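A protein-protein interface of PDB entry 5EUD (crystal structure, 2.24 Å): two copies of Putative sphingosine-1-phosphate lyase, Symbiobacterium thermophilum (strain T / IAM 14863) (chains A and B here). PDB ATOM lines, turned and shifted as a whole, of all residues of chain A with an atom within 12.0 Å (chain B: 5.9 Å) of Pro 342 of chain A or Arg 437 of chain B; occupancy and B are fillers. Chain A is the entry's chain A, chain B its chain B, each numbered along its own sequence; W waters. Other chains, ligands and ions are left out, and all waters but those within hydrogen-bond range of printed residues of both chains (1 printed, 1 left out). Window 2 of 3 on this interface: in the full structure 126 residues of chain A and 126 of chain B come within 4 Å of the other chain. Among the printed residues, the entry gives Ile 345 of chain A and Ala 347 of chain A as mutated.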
ATOM      1  N   PHE A 336     -20.576  -0.846 -18.942  1.00  0.00           N
ATOM      2  CA  PHE A 336     -19.902   0.295 -19.562  1.00  0.00           C
ATOM      3  C   PHE A 336     -21.021   1.212 -20.065  1.00  0.00           C
ATOM      4  O   PHE A 336     -21.952   0.729 -20.700  1.00  0.00           O
ATOM      5  CB  PHE A 336     -18.935  -0.109 -20.714  1.00  0.00           C
ATOM      6  CG  PHE A 336     -18.620   1.066 -21.620  1.00  0.00           C
ATOM      7  CD1 PHE A 336     -17.689   2.023 -21.244  1.00  0.00           C
ATOM      8  CD2 PHE A 336     -19.319   1.255 -22.816  1.00  0.00           C
ATOM      9  CE1 PHE A 336     -17.471   3.160 -22.026  1.00  0.00           C
ATOM     10  CE2 PHE A 336     -19.072   2.375 -23.621  1.00  0.00           C
ATOM     11  CZ  PHE A 336     -18.140   3.309 -23.225  1.00  0.00           C
ATOM     12  N   ILE A 337     -20.975   2.511 -19.714  1.00  0.00           N
ATOM     13  CA  ILE A 337     -21.999   3.471 -20.156  1.00  0.00           C
ATOM     14  C   ILE A 337     -21.327   4.723 -20.764  1.00  0.00           C
ATOM     15  O   ILE A 337     -20.479   5.334 -20.113  1.00  0.00           O
ATOM     16  CB  ILE A 337     -23.044   3.820 -19.040  1.00  0.00           C
ATOM     17  CG1 ILE A 337     -23.850   2.571 -18.592  1.00  0.00           C
ATOM     18  CG2 ILE A 337     -24.016   4.887 -19.514  1.00  0.00           C
ATOM     19  CD1 ILE A 337     -23.915   2.378 -17.106  1.00  0.00           C
ATOM     20  N   ALA A 338     -21.677   5.070 -22.020  1.00  0.00           N
ATOM     21  CA  ALA A 338     -21.169   6.269 -22.695  1.00  0.00           C
ATOM     22  C   ALA A 338     -22.337   7.229 -22.803  1.00  0.00           C
ATOM     23  O   ALA A 338     -23.361   6.899 -23.409  1.00  0.00           O
ATOM     24  CB  ALA A 338     -20.614   5.939 -24.073  1.00  0.00           C
ATOM     25  N   ALA A 339     -22.184   8.410 -22.178  1.00  0.00           N
ATOM     26  CA  ALA A 339     -23.206   9.457 -22.067  1.00  0.00           C
ATOM     27  C   ALA A 339     -23.068  10.651 -23.019  1.00  0.00           C
ATOM     28  O   ALA A 339     -24.048  11.355 -23.230  1.00  0.00           O
ATOM     29  CB  ALA A 339     -23.241   9.959 -20.626  1.00  0.00           C
ATOM     30  N   ASP A 340     -21.876  10.899 -23.569  1.00  0.00           N
ATOM     31  CA  ASP A 340     -21.579  12.071 -24.406  1.00  0.00           C
ATOM     32  C   ASP A 340     -21.267  11.752 -25.885  1.00  0.00           C
ATOM     33  O   ASP A 340     -20.855  12.630 -26.639  1.00  0.00           O
ATOM     34  CB  ASP A 340     -20.415  12.890 -23.764  1.00  0.00           C
ATOM     35  CG  ASP A 340     -20.627  13.287 -22.308  1.00  0.00           C
ATOM     36  OD1 ASP A 340     -21.735  13.776 -21.975  1.00  0.00           O
ATOM     37  OD2 ASP A 340     -19.672  13.144 -21.509  1.00  0.00           O
ATOM     38  N   TRP A 341     -21.478  10.514 -26.301  1.00  0.00           N
ATOM     39  CA  TRP A 341     -21.200  10.117 -27.683  1.00  0.00           C
ATOM     40  C   TRP A 341     -22.317  10.591 -28.633  1.00  0.00           C
ATOM     41  O   TRP A 341     -23.485  10.245 -28.403  1.00  0.00           O
ATOM     42  CB  TRP A 341     -21.021   8.595 -27.755  1.00  0.00           C
ATOM     43  CG  TRP A 341     -20.686   8.043 -29.112  1.00  0.00           C
ATOM     44  CD1 TRP A 341     -19.702   8.473 -29.960  1.00  0.00           C
ATOM     45  CD2 TRP A 341     -21.242   6.860 -29.710  1.00  0.00           C
ATOM     46  NE1 TRP A 341     -19.674   7.682 -31.087  1.00  0.00           N
ATOM     47  CE2 TRP A 341     -20.589   6.667 -30.946  1.00  0.00           C
ATOM     48  CE3 TRP A 341     -22.239   5.943 -29.318  1.00  0.00           C
ATOM     49  CZ2 TRP A 341     -20.912   5.606 -31.809  1.00  0.00           C
ATOM     50  CZ3 TRP A 341     -22.537   4.875 -30.157  1.00  0.00           C
ATOM     51  CH2 TRP A 341     -21.882   4.720 -31.391  1.00  0.00           C
ATOM     52  N   PRO A 342     -21.995  11.302 -29.743  1.00  0.00           N
ATOM     53  CA  PRO A 342     -23.057  11.700 -30.694  1.00  0.00           C
ATOM     54  C   PRO A 342     -23.836  10.534 -31.325  1.00  0.00           C
ATOM     55  O   PRO A 342     -24.904  10.758 -31.889  1.00  0.00           O
ATOM     56  CB  PRO A 342     -22.315  12.544 -31.752  1.00  0.00           C
ATOM     57  CG  PRO A 342     -21.057  12.943 -31.116  1.00  0.00           C
ATOM     58  CD  PRO A 342     -20.686  11.838 -30.159  1.00  0.00           C
ATOM     59  N   GLY A 343     -23.335   9.306 -31.192  1.00  0.00           N
ATOM     60  CA  GLY A 343     -24.020   8.112 -31.687  1.00  0.00           C
ATOM     61  C   GLY A 343     -25.178   7.665 -30.811  1.00  0.00           C
ATOM     62  O   GLY A 343     -25.812   6.636 -31.089  1.00  0.00           O
ATOM     63  N   GLY A 344     -25.440   8.448 -29.760  1.00  0.00           N
ATOM     64  CA  GLY A 344     -26.494   8.235 -28.778  1.00  0.00           C
ATOM     65  C   GLY A 344     -25.982   7.657 -27.473  1.00  0.00           C
ATOM     66  O   GLY A 344     -24.796   7.327 -27.359  1.00  0.00           O
ATOM     67  N   ILE A 345     -26.885   7.517 -26.483  1.00  0.00           N
ATOM     68  CA  ILE A 345     -26.584   6.880 -25.199  1.00  0.00           C
ATOM     69  C   ILE A 345     -26.282   5.394 -25.484  1.00  0.00           C
ATOM     70  O   ILE A 345     -27.068   4.714 -26.129  1.00  0.00           O
ATOM     71  CB  ILE A 345     -27.717   7.074 -24.150  1.00  0.00           C
ATOM     72  CG1 ILE A 345     -27.801   8.566 -23.752  1.00  0.00           C
ATOM     73  CG2 ILE A 345     -27.465   6.192 -22.901  1.00  0.00           C
ATOM     74  CD1 ILE A 345     -29.114   8.997 -23.230  1.00  0.00           C
ATOM     75  N   TYR A 346     -25.123   4.925 -25.019  1.00  0.00           N
ATOM     76  CA  TYR A 346     -24.637   3.594 -25.266  1.00  0.00           C
ATOM     77  C   TYR A 346     -24.329   2.905 -23.945  1.00  0.00           C
ATOM     78  O   TYR A 346     -23.687   3.480 -23.073  1.00  0.00           O
ATOM     79  CB  TYR A 346     -23.393   3.706 -26.160  1.00  0.00           C
ATOM     80  CG  TYR A 346     -22.940   2.395 -26.739  1.00  0.00           C
ATOM     81  CD1 TYR A 346     -23.436   1.942 -27.955  1.00  0.00           C
ATOM     82  CD2 TYR A 346     -21.966   1.631 -26.102  1.00  0.00           C
ATOM     83  CE1 TYR A 346     -22.993   0.747 -28.516  1.00  0.00           C
ATOM     84  CE2 TYR A 346     -21.516   0.435 -26.650  1.00  0.00           C
ATOM     85  CZ  TYR A 346     -22.039  -0.010 -27.853  1.00  0.00           C
ATOM     86  OH  TYR A 346     -21.608  -1.199 -28.392  1.00  0.00           O
ATOM     87  N   ALA A 347     -24.803   1.677 -23.803  1.00  0.00           N
ATOM     88  CA  ALA A 347     -24.680   0.878 -22.584  1.00  0.00           C
ATOM     89  C   ALA A 347     -24.393  -0.595 -22.914  1.00  0.00           C
ATOM     90  O   ALA A 347     -25.164  -1.213 -23.636  1.00  0.00           O
ATOM     91  CB  ALA A 347     -25.969   0.995 -21.776  1.00  0.00           C
ATOM     92  N   VAL B 199     -14.597  13.207 -31.697  1.00  0.00           N
ATOM     93  CA  VAL B 199     -15.755  13.008 -30.801  1.00  0.00           C
ATOM     94  C   VAL B 199     -16.763  11.978 -31.349  1.00  0.00           C
ATOM     95  O   VAL B 199     -17.398  11.272 -30.573  1.00  0.00           O
ATOM     96  CB  VAL B 199     -16.464  14.322 -30.386  1.00  0.00           C
ATOM     97  CG1 VAL B 199     -15.632  15.078 -29.380  1.00  0.00           C
ATOM     98  CG2 VAL B 199     -16.800  15.207 -31.594  1.00  0.00           C
ATOM     99  N   SER B 200     -16.858  11.878 -32.677  1.00  0.00           N
ATOM    100  CA  SER B 200     -17.724  10.967 -33.418  1.00  0.00           C
ATOM    101  C   SER B 200     -17.248   9.490 -33.423  1.00  0.00           C
ATOM    102  O   SER B 200     -17.999   8.622 -33.866  1.00  0.00           O
ATOM    103  CB  SER B 200     -17.840  11.456 -34.860  1.00  0.00           C
ATOM    104  OG  SER B 200     -16.616  11.273 -35.551  1.00  0.00           O
ATOM    105  N   ARG B 218     -10.888  13.188 -26.871  1.00  0.00           N
ATOM    106  CA  ARG B 218     -11.851  13.342 -27.958  1.00  0.00           C
ATOM    107  C   ARG B 218     -11.779  14.758 -28.528  1.00  0.00           C
ATOM    108  O   ARG B 218     -11.885  15.728 -27.780  1.00  0.00           O
ATOM    109  CB  ARG B 218     -13.261  12.952 -27.497  1.00  0.00           C
ATOM    110  CG  ARG B 218     -13.388  11.452 -27.285  1.00  0.00           C
ATOM    111  CD  ARG B 218     -14.813  11.036 -27.047  1.00  0.00           C
ATOM    112  NE  ARG B 218     -14.974   9.579 -27.116  1.00  0.00           N
ATOM    113  CZ  ARG B 218     -15.259   8.898 -28.225  1.00  0.00           C
ATOM    114  NH1 ARG B 218     -15.422   9.528 -29.378  1.00  0.00           N
ATOM    115  NH2 ARG B 218     -15.391   7.585 -28.184  1.00  0.00           N
ATOM    116  N   LEU B 221     -15.291  18.308 -34.246  1.00  0.00           N
ATOM    117  CA  LEU B 221     -15.496  18.139 -35.675  1.00  0.00           C
ATOM    118  C   LEU B 221     -15.529  19.492 -36.386  1.00  0.00           C
ATOM    119  O   LEU B 221     -15.670  20.530 -35.736  1.00  0.00           O
ATOM    120  CB  LEU B 221     -16.810  17.376 -35.926  1.00  0.00           C
ATOM    121  CG  LEU B 221     -17.015  16.028 -35.192  1.00  0.00           C
ATOM    122  CD1 LEU B 221     -18.387  15.450 -35.488  1.00  0.00           C
ATOM    123  CD2 LEU B 221     -15.868  15.037 -35.468  1.00  0.00           C
ATOM    124  N   TYR B 225     -18.920  17.835 -40.176  1.00  0.00           N
ATOM    125  CA  TYR B 225     -19.029  16.733 -39.205  1.00  0.00           C
ATOM    126  C   TYR B 225     -17.874  15.726 -39.371  1.00  0.00           C
ATOM    127  O   TYR B 225     -17.954  14.590 -38.918  1.00  0.00           O
ATOM    128  CB  TYR B 225     -20.429  16.073 -39.240  1.00  0.00           C
ATOM    129  CG  TYR B 225     -21.514  17.013 -38.763  1.00  0.00           C
ATOM    130  CD1 TYR B 225     -22.163  17.869 -39.651  1.00  0.00           C
ATOM    131  CD2 TYR B 225     -21.891  17.055 -37.420  1.00  0.00           C
ATOM    132  CE1 TYR B 225     -23.134  18.764 -39.213  1.00  0.00           C
ATOM    133  CE2 TYR B 225     -22.866  17.949 -36.969  1.00  0.00           C
ATOM    134  CZ  TYR B 225     -23.483  18.802 -37.872  1.00  0.00           C
ATOM    135  OH  TYR B 225     -24.461  19.670 -37.458  1.00  0.00           O
ATOM    136  N   PRO B 251     -22.274   7.794 -36.149  1.00  0.00           N
ATOM    137  CA  PRO B 251     -23.334   8.790 -35.967  1.00  0.00           C
ATOM    138  C   PRO B 251     -23.883   9.407 -37.242  1.00  0.00           C
ATOM    139  O   PRO B 251     -25.086   9.296 -37.503  1.00  0.00           O
ATOM    140  CB  PRO B 251     -22.702   9.826 -35.031  1.00  0.00           C
ATOM    141  CG  PRO B 251     -21.655   9.075 -34.293  1.00  0.00           C
ATOM    142  CD  PRO B 251     -21.105   8.113 -35.294  1.00  0.00           C
ATOM    143  N   HIS B 252     -22.998   9.986 -38.060  1.00  0.00           N
ATOM    144  CA  HIS B 252     -23.370  10.750 -39.233  1.00  0.00           C
ATOM    145  C   HIS B 252     -22.940  10.137 -40.581  1.00  0.00           C
ATOM    146  O   HIS B 252     -23.195  10.736 -41.639  1.00  0.00           O
ATOM    147  CB  HIS B 252     -22.846  12.180 -39.048  1.00  0.00           C
ATOM    148  CG  HIS B 252     -23.211  12.763 -37.712  1.00  0.00           C
ATOM    149  ND1 HIS B 252     -22.296  13.470 -36.964  1.00  0.00           N
ATOM    150  CD2 HIS B 252     -24.375  12.689 -37.018  1.00  0.00           C
ATOM    151  CE1 HIS B 252     -22.930  13.835 -35.852  1.00  0.00           C
ATOM    152  NE2 HIS B 252     -24.185  13.397 -35.842  1.00  0.00           N
ATOM    153  N   TYR B 419     -36.816  14.722 -32.533  1.00  0.00           N
ATOM    154  CA  TYR B 419     -37.243  13.588 -31.700  1.00  0.00           C
ATOM    155  C   TYR B 419     -38.741  13.284 -31.892  1.00  0.00           C
ATOM    156  O   TYR B 419     -39.121  12.118 -31.831  1.00  0.00           O
ATOM    157  CB  TYR B 419     -36.885  13.836 -30.238  1.00  0.00           C
ATOM    158  CG  TYR B 419     -35.399  13.849 -29.961  1.00  0.00           C
ATOM    159  CD1 TYR B 419     -34.537  12.962 -30.610  1.00  0.00           C
ATOM    160  CD2 TYR B 419     -34.866  14.662 -28.972  1.00  0.00           C
ATOM    161  CE1 TYR B 419     -33.172  12.940 -30.327  1.00  0.00           C
ATOM    162  CE2 TYR B 419     -33.501  14.653 -28.683  1.00  0.00           C
ATOM    163  CZ  TYR B 419     -32.660  13.781 -29.355  1.00  0.00           C
ATOM    164  OH  TYR B 419     -31.322  13.754 -29.045  1.00  0.00           O
ATOM    165  N   GLY B 434     -31.755   6.954 -32.585  1.00  0.00           N
ATOM    166  CA  GLY B 434     -31.795   8.288 -31.993  1.00  0.00           C
ATOM    167  C   GLY B 434     -30.410   8.757 -31.590  1.00  0.00           C
ATOM    168  O   GLY B 434     -29.686   8.052 -30.881  1.00  0.00           O
ATOM    169  N   LEU B 435     -30.029   9.944 -32.036  1.00  0.00           N
ATOM    170  CA  LEU B 435     -28.713  10.517 -31.778  1.00  0.00           C
ATOM    171  C   LEU B 435     -28.864  11.792 -30.978  1.00  0.00           C
ATOM    172  O   LEU B 435     -29.971  12.324 -30.869  1.00  0.00           O
ATOM    173  CB  LEU B 435     -27.993  10.821 -33.112  1.00  0.00           C
ATOM    174  CG  LEU B 435     -27.975   9.742 -34.213  1.00  0.00           C
ATOM    175  CD1 LEU B 435     -27.615  10.346 -35.557  1.00  0.00           C
ATOM    176  CD2 LEU B 435     -27.011   8.600 -33.875  1.00  0.00           C
ATOM    177  N   HIS B 436     -27.766  12.256 -30.378  1.00  0.00           N
ATOM    178  CA  HIS B 436     -27.735  13.515 -29.633  1.00  0.00           C
ATOM    179  C   HIS B 436     -26.395  14.172 -29.903  1.00  0.00           C
ATOM    180  O   HIS B 436     -25.566  13.558 -30.591  1.00  0.00           O
ATOM    181  CB  HIS B 436     -28.091  13.351 -28.132  1.00  0.00           C
ATOM    182  CG  HIS B 436     -27.050  12.713 -27.249  1.00  0.00           C
ATOM    183  ND1 HIS B 436     -26.230  11.686 -27.696  1.00  0.00           N
ATOM    184  CD2 HIS B 436     -26.788  12.931 -25.943  1.00  0.00           C
ATOM    185  CE1 HIS B 436     -25.482  11.348 -26.660  1.00  0.00           C
ATOM    186  NE2 HIS B 436     -25.786  12.064 -25.586  1.00  0.00           N
ATOM    187  N   ARG B 437     -26.212  15.442 -29.470  1.00  0.00           N
ATOM    188  CA  ARG B 437     -24.980  16.206 -29.717  1.00  0.00           C
ATOM    189  C   ARG B 437     -24.601  16.253 -31.232  1.00  0.00           C
ATOM    190  O   ARG B 437     -23.517  15.797 -31.597  1.00  0.00           O
ATOM    191  CB  ARG B 437     -23.822  15.648 -28.846  1.00  0.00           C
ATOM    192  CG  ARG B 437     -23.916  16.086 -27.403  1.00  0.00           C
ATOM    193  CD  ARG B 437     -23.027  15.235 -26.521  1.00  0.00           C
ATOM    194  NE  ARG B 437     -22.577  15.950 -25.322  1.00  0.00           N
ATOM    195  CZ  ARG B 437     -23.290  16.091 -24.208  1.00  0.00           C
ATOM    196  NH1 ARG B 437     -24.518  15.589 -24.126  1.00  0.00           N
ATOM    197  NH2 ARG B 437     -22.786  16.750 -23.172  1.00  0.00           N
ATOM    198  N   PRO B 438     -25.483  16.736 -32.143  1.00  0.00           N
ATOM    199  CA  PRO B 438     -26.796  17.380 -31.903  1.00  0.00           C
ATOM    200  C   PRO B 438     -28.010  16.441 -31.951  1.00  0.00           C
ATOM    201  O   PRO B 438     -27.913  15.368 -32.545  1.00  0.00           O
ATOM    202  CB  PRO B 438     -26.867  18.398 -33.051  1.00  0.00           C
ATOM    203  CG  PRO B 438     -26.212  17.660 -34.210  1.00  0.00           C
ATOM    204  CD  PRO B 438     -25.120  16.787 -33.577  1.00  0.00           C
ATOM    205  N   PRO B 439     -29.198  16.831 -31.430  1.00  0.00           N
ATOM    206  CA  PRO B 439     -30.376  15.964 -31.607  1.00  0.00           C
ATOM    207  C   PRO B 439     -30.576  15.680 -33.102  1.00  0.00           C
ATOM    208  O   PRO B 439     -30.472  16.590 -33.939  1.00  0.00           O
ATOM    209  CB  PRO B 439     -31.516  16.816 -31.044  1.00  0.00           C
ATOM    210  CG  PRO B 439     -30.833  17.693 -29.995  1.00  0.00           C
ATOM    211  CD  PRO B 439     -29.550  18.059 -30.687  1.00  0.00           C
ATOM    212  N   ALA B 487     -31.099  13.788 -23.753  1.00  0.00           N
ATOM    213  CA  ALA B 487     -30.165  14.711 -24.413  1.00  0.00           C
ATOM    214  C   ALA B 487     -29.869  15.928 -23.504  1.00  0.00           C
ATOM    215  O   ALA B 487     -28.786  16.498 -23.586  1.00  0.00           O
ATOM    216  CB  ALA B 487     -30.739  15.180 -25.740  1.00  0.00           C
ATOM    217  N   ALA B 489     -30.172  15.737 -19.938  1.00  0.00           N
ATOM    218  CA  ALA B 489     -29.767  15.167 -18.646  1.00  0.00           C
ATOM    219  C   ALA B 489     -28.277  15.274 -18.280  1.00  0.00           C
ATOM    220  O   ALA B 489     -27.424  15.147 -19.162  1.00  0.00           O
ATOM    221  CB  ALA B 489     -30.200  13.709 -18.568  1.00  0.00           C
HETATM  222  O   HOH W   1     -28.340   5.812 -31.627  1.00  0.00           O
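The backbone carbonyl oxygen (O) of Trp 341 of chain A sits close to a ring nitrogen (ND1) of His 436 of chain B. The indole nitrogen of Trp 341 of chain A sits at hydrogen-bond distance from the backbone carbonyl oxygen of Ser 200 of chain B. The guanidinium group (NH2) of Arg 437 of chain B lies within salt-bridge range of the side-chain carboxylate (OD1) of Asp 340 of chain A, at 3.4 Å. O of Ala 339 of chain A lies within hydrogen-bond range of NE2 of His 436 of chain B (3.0 Å). The backbone carbonyl oxygen of Pro 342 of chain A lies close to the backbone carbonyl oxygen of His 436 of chain B (3.2 Å).
O of Val 199 of chain B is in hydrogen-bond range of NH1 of Arg 218 of chain B, at 2.9 Å. The backbone carbonyl oxygen (O) of Leu 435 of chain B sits at hydrogen-bond distance from the side-chain hydroxyl (OH) of Tyr 419 of chain B, at 2.7 Å.
Among the printed residues, merely in contact across the chains: Trp 341 of chain A with Val 199 of chain B, Pro 342 of chain A with Val 199 of chain B, Pro 342 of chain A with Pro 251 of chain B, Pro 342 of chain A with Leu 435 of chain B, Pro 342 of chain A with Arg 437 of chain B, Gly 343 of chain A with Pro 251 of chain B, Gly 343 of chain A with Leu 435 of chain B, Gly 344 of chain A with Gly 434 of chain B and Gly 344 of chain A with His 436 of chain B.
Printed residues of chain B within 4 Å of Pro 342 of chain A: Val 199 (3.4 Å), Pro 251 (3.9 Å), Leu 435 (3.3 Å), His 436 (3.1 Å) and Arg 437 (3.5 Å). Arg 437 of chain B touches just these residues of chain A: Asp 340 (3.4 Å) and Pro 342 (3.5 Å). Of chain A, only Trp 341 and Pro 342 come within 4 Å of Val 199 of chain B. Of chain A, only Trp 341 (3.4 Å) comes within 4 Å of Ser 200 of chain B. Gly 434 of chain B touches just one residue of chain A: Gly 344 (3.8 Å). His 436 of chain B touches four residues of chain A. No residue of chain A comes within 4 Å of Pro 439 of chain B. No residue of chain A comes within 4 Å of Ala 487 of chain B. Of the printed residues of chain B, Trp 341 of chain A touches Val 199 (3.7 Å), Ser 200 (3.4 Å) and His 436 (2.9 Å). Of the printed residues of chain B, Asp 340 of chain A touches Arg 437 (3.4 Å). Printed residues of chain B within 4 Å of Gly 344 of chain A: Gly 434 (3.8 Å) and His 436 (3.6 Å). Of the printed residues of chain B, Ala 339 of chain A touches His 436 (3.0 Å). Printed residues of chain B within 4 Å of Gly 343 of chain A: Pro 251 (3.5 Å) and Leu 435 (3.6 Å). Ile 337 of chain A touches none of the printed residues of chain B. Arg 218 of chain B touches none of the printed residues of chain A. The nearest residue of chain B that does not touch Pro 342 of chain A is His 252 of chain B (4.3 Å). The nearest printed residue of chain A that does not touch Pro 251 of chain B is Trp 341 of chain A (4.02 Å).
Hydrophobic or aromatic side chains of chain B that line the printed part of chain A: Pro 251, Leu 435 and His 436. Hydrophobic or aromatic side chains of chain A within 4 Å of the printed part of chain B: Trp 341 and Pro 342.
No position is printed for both chains. Of the 14 pairs that touch across the chains among the printed residues, none has its exchanged pair printed and touching as well.
Water W1 bridges O of Gly 343 of chain A (2.7 Å) and O of Gly 434 of chain B (2.7 Å).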
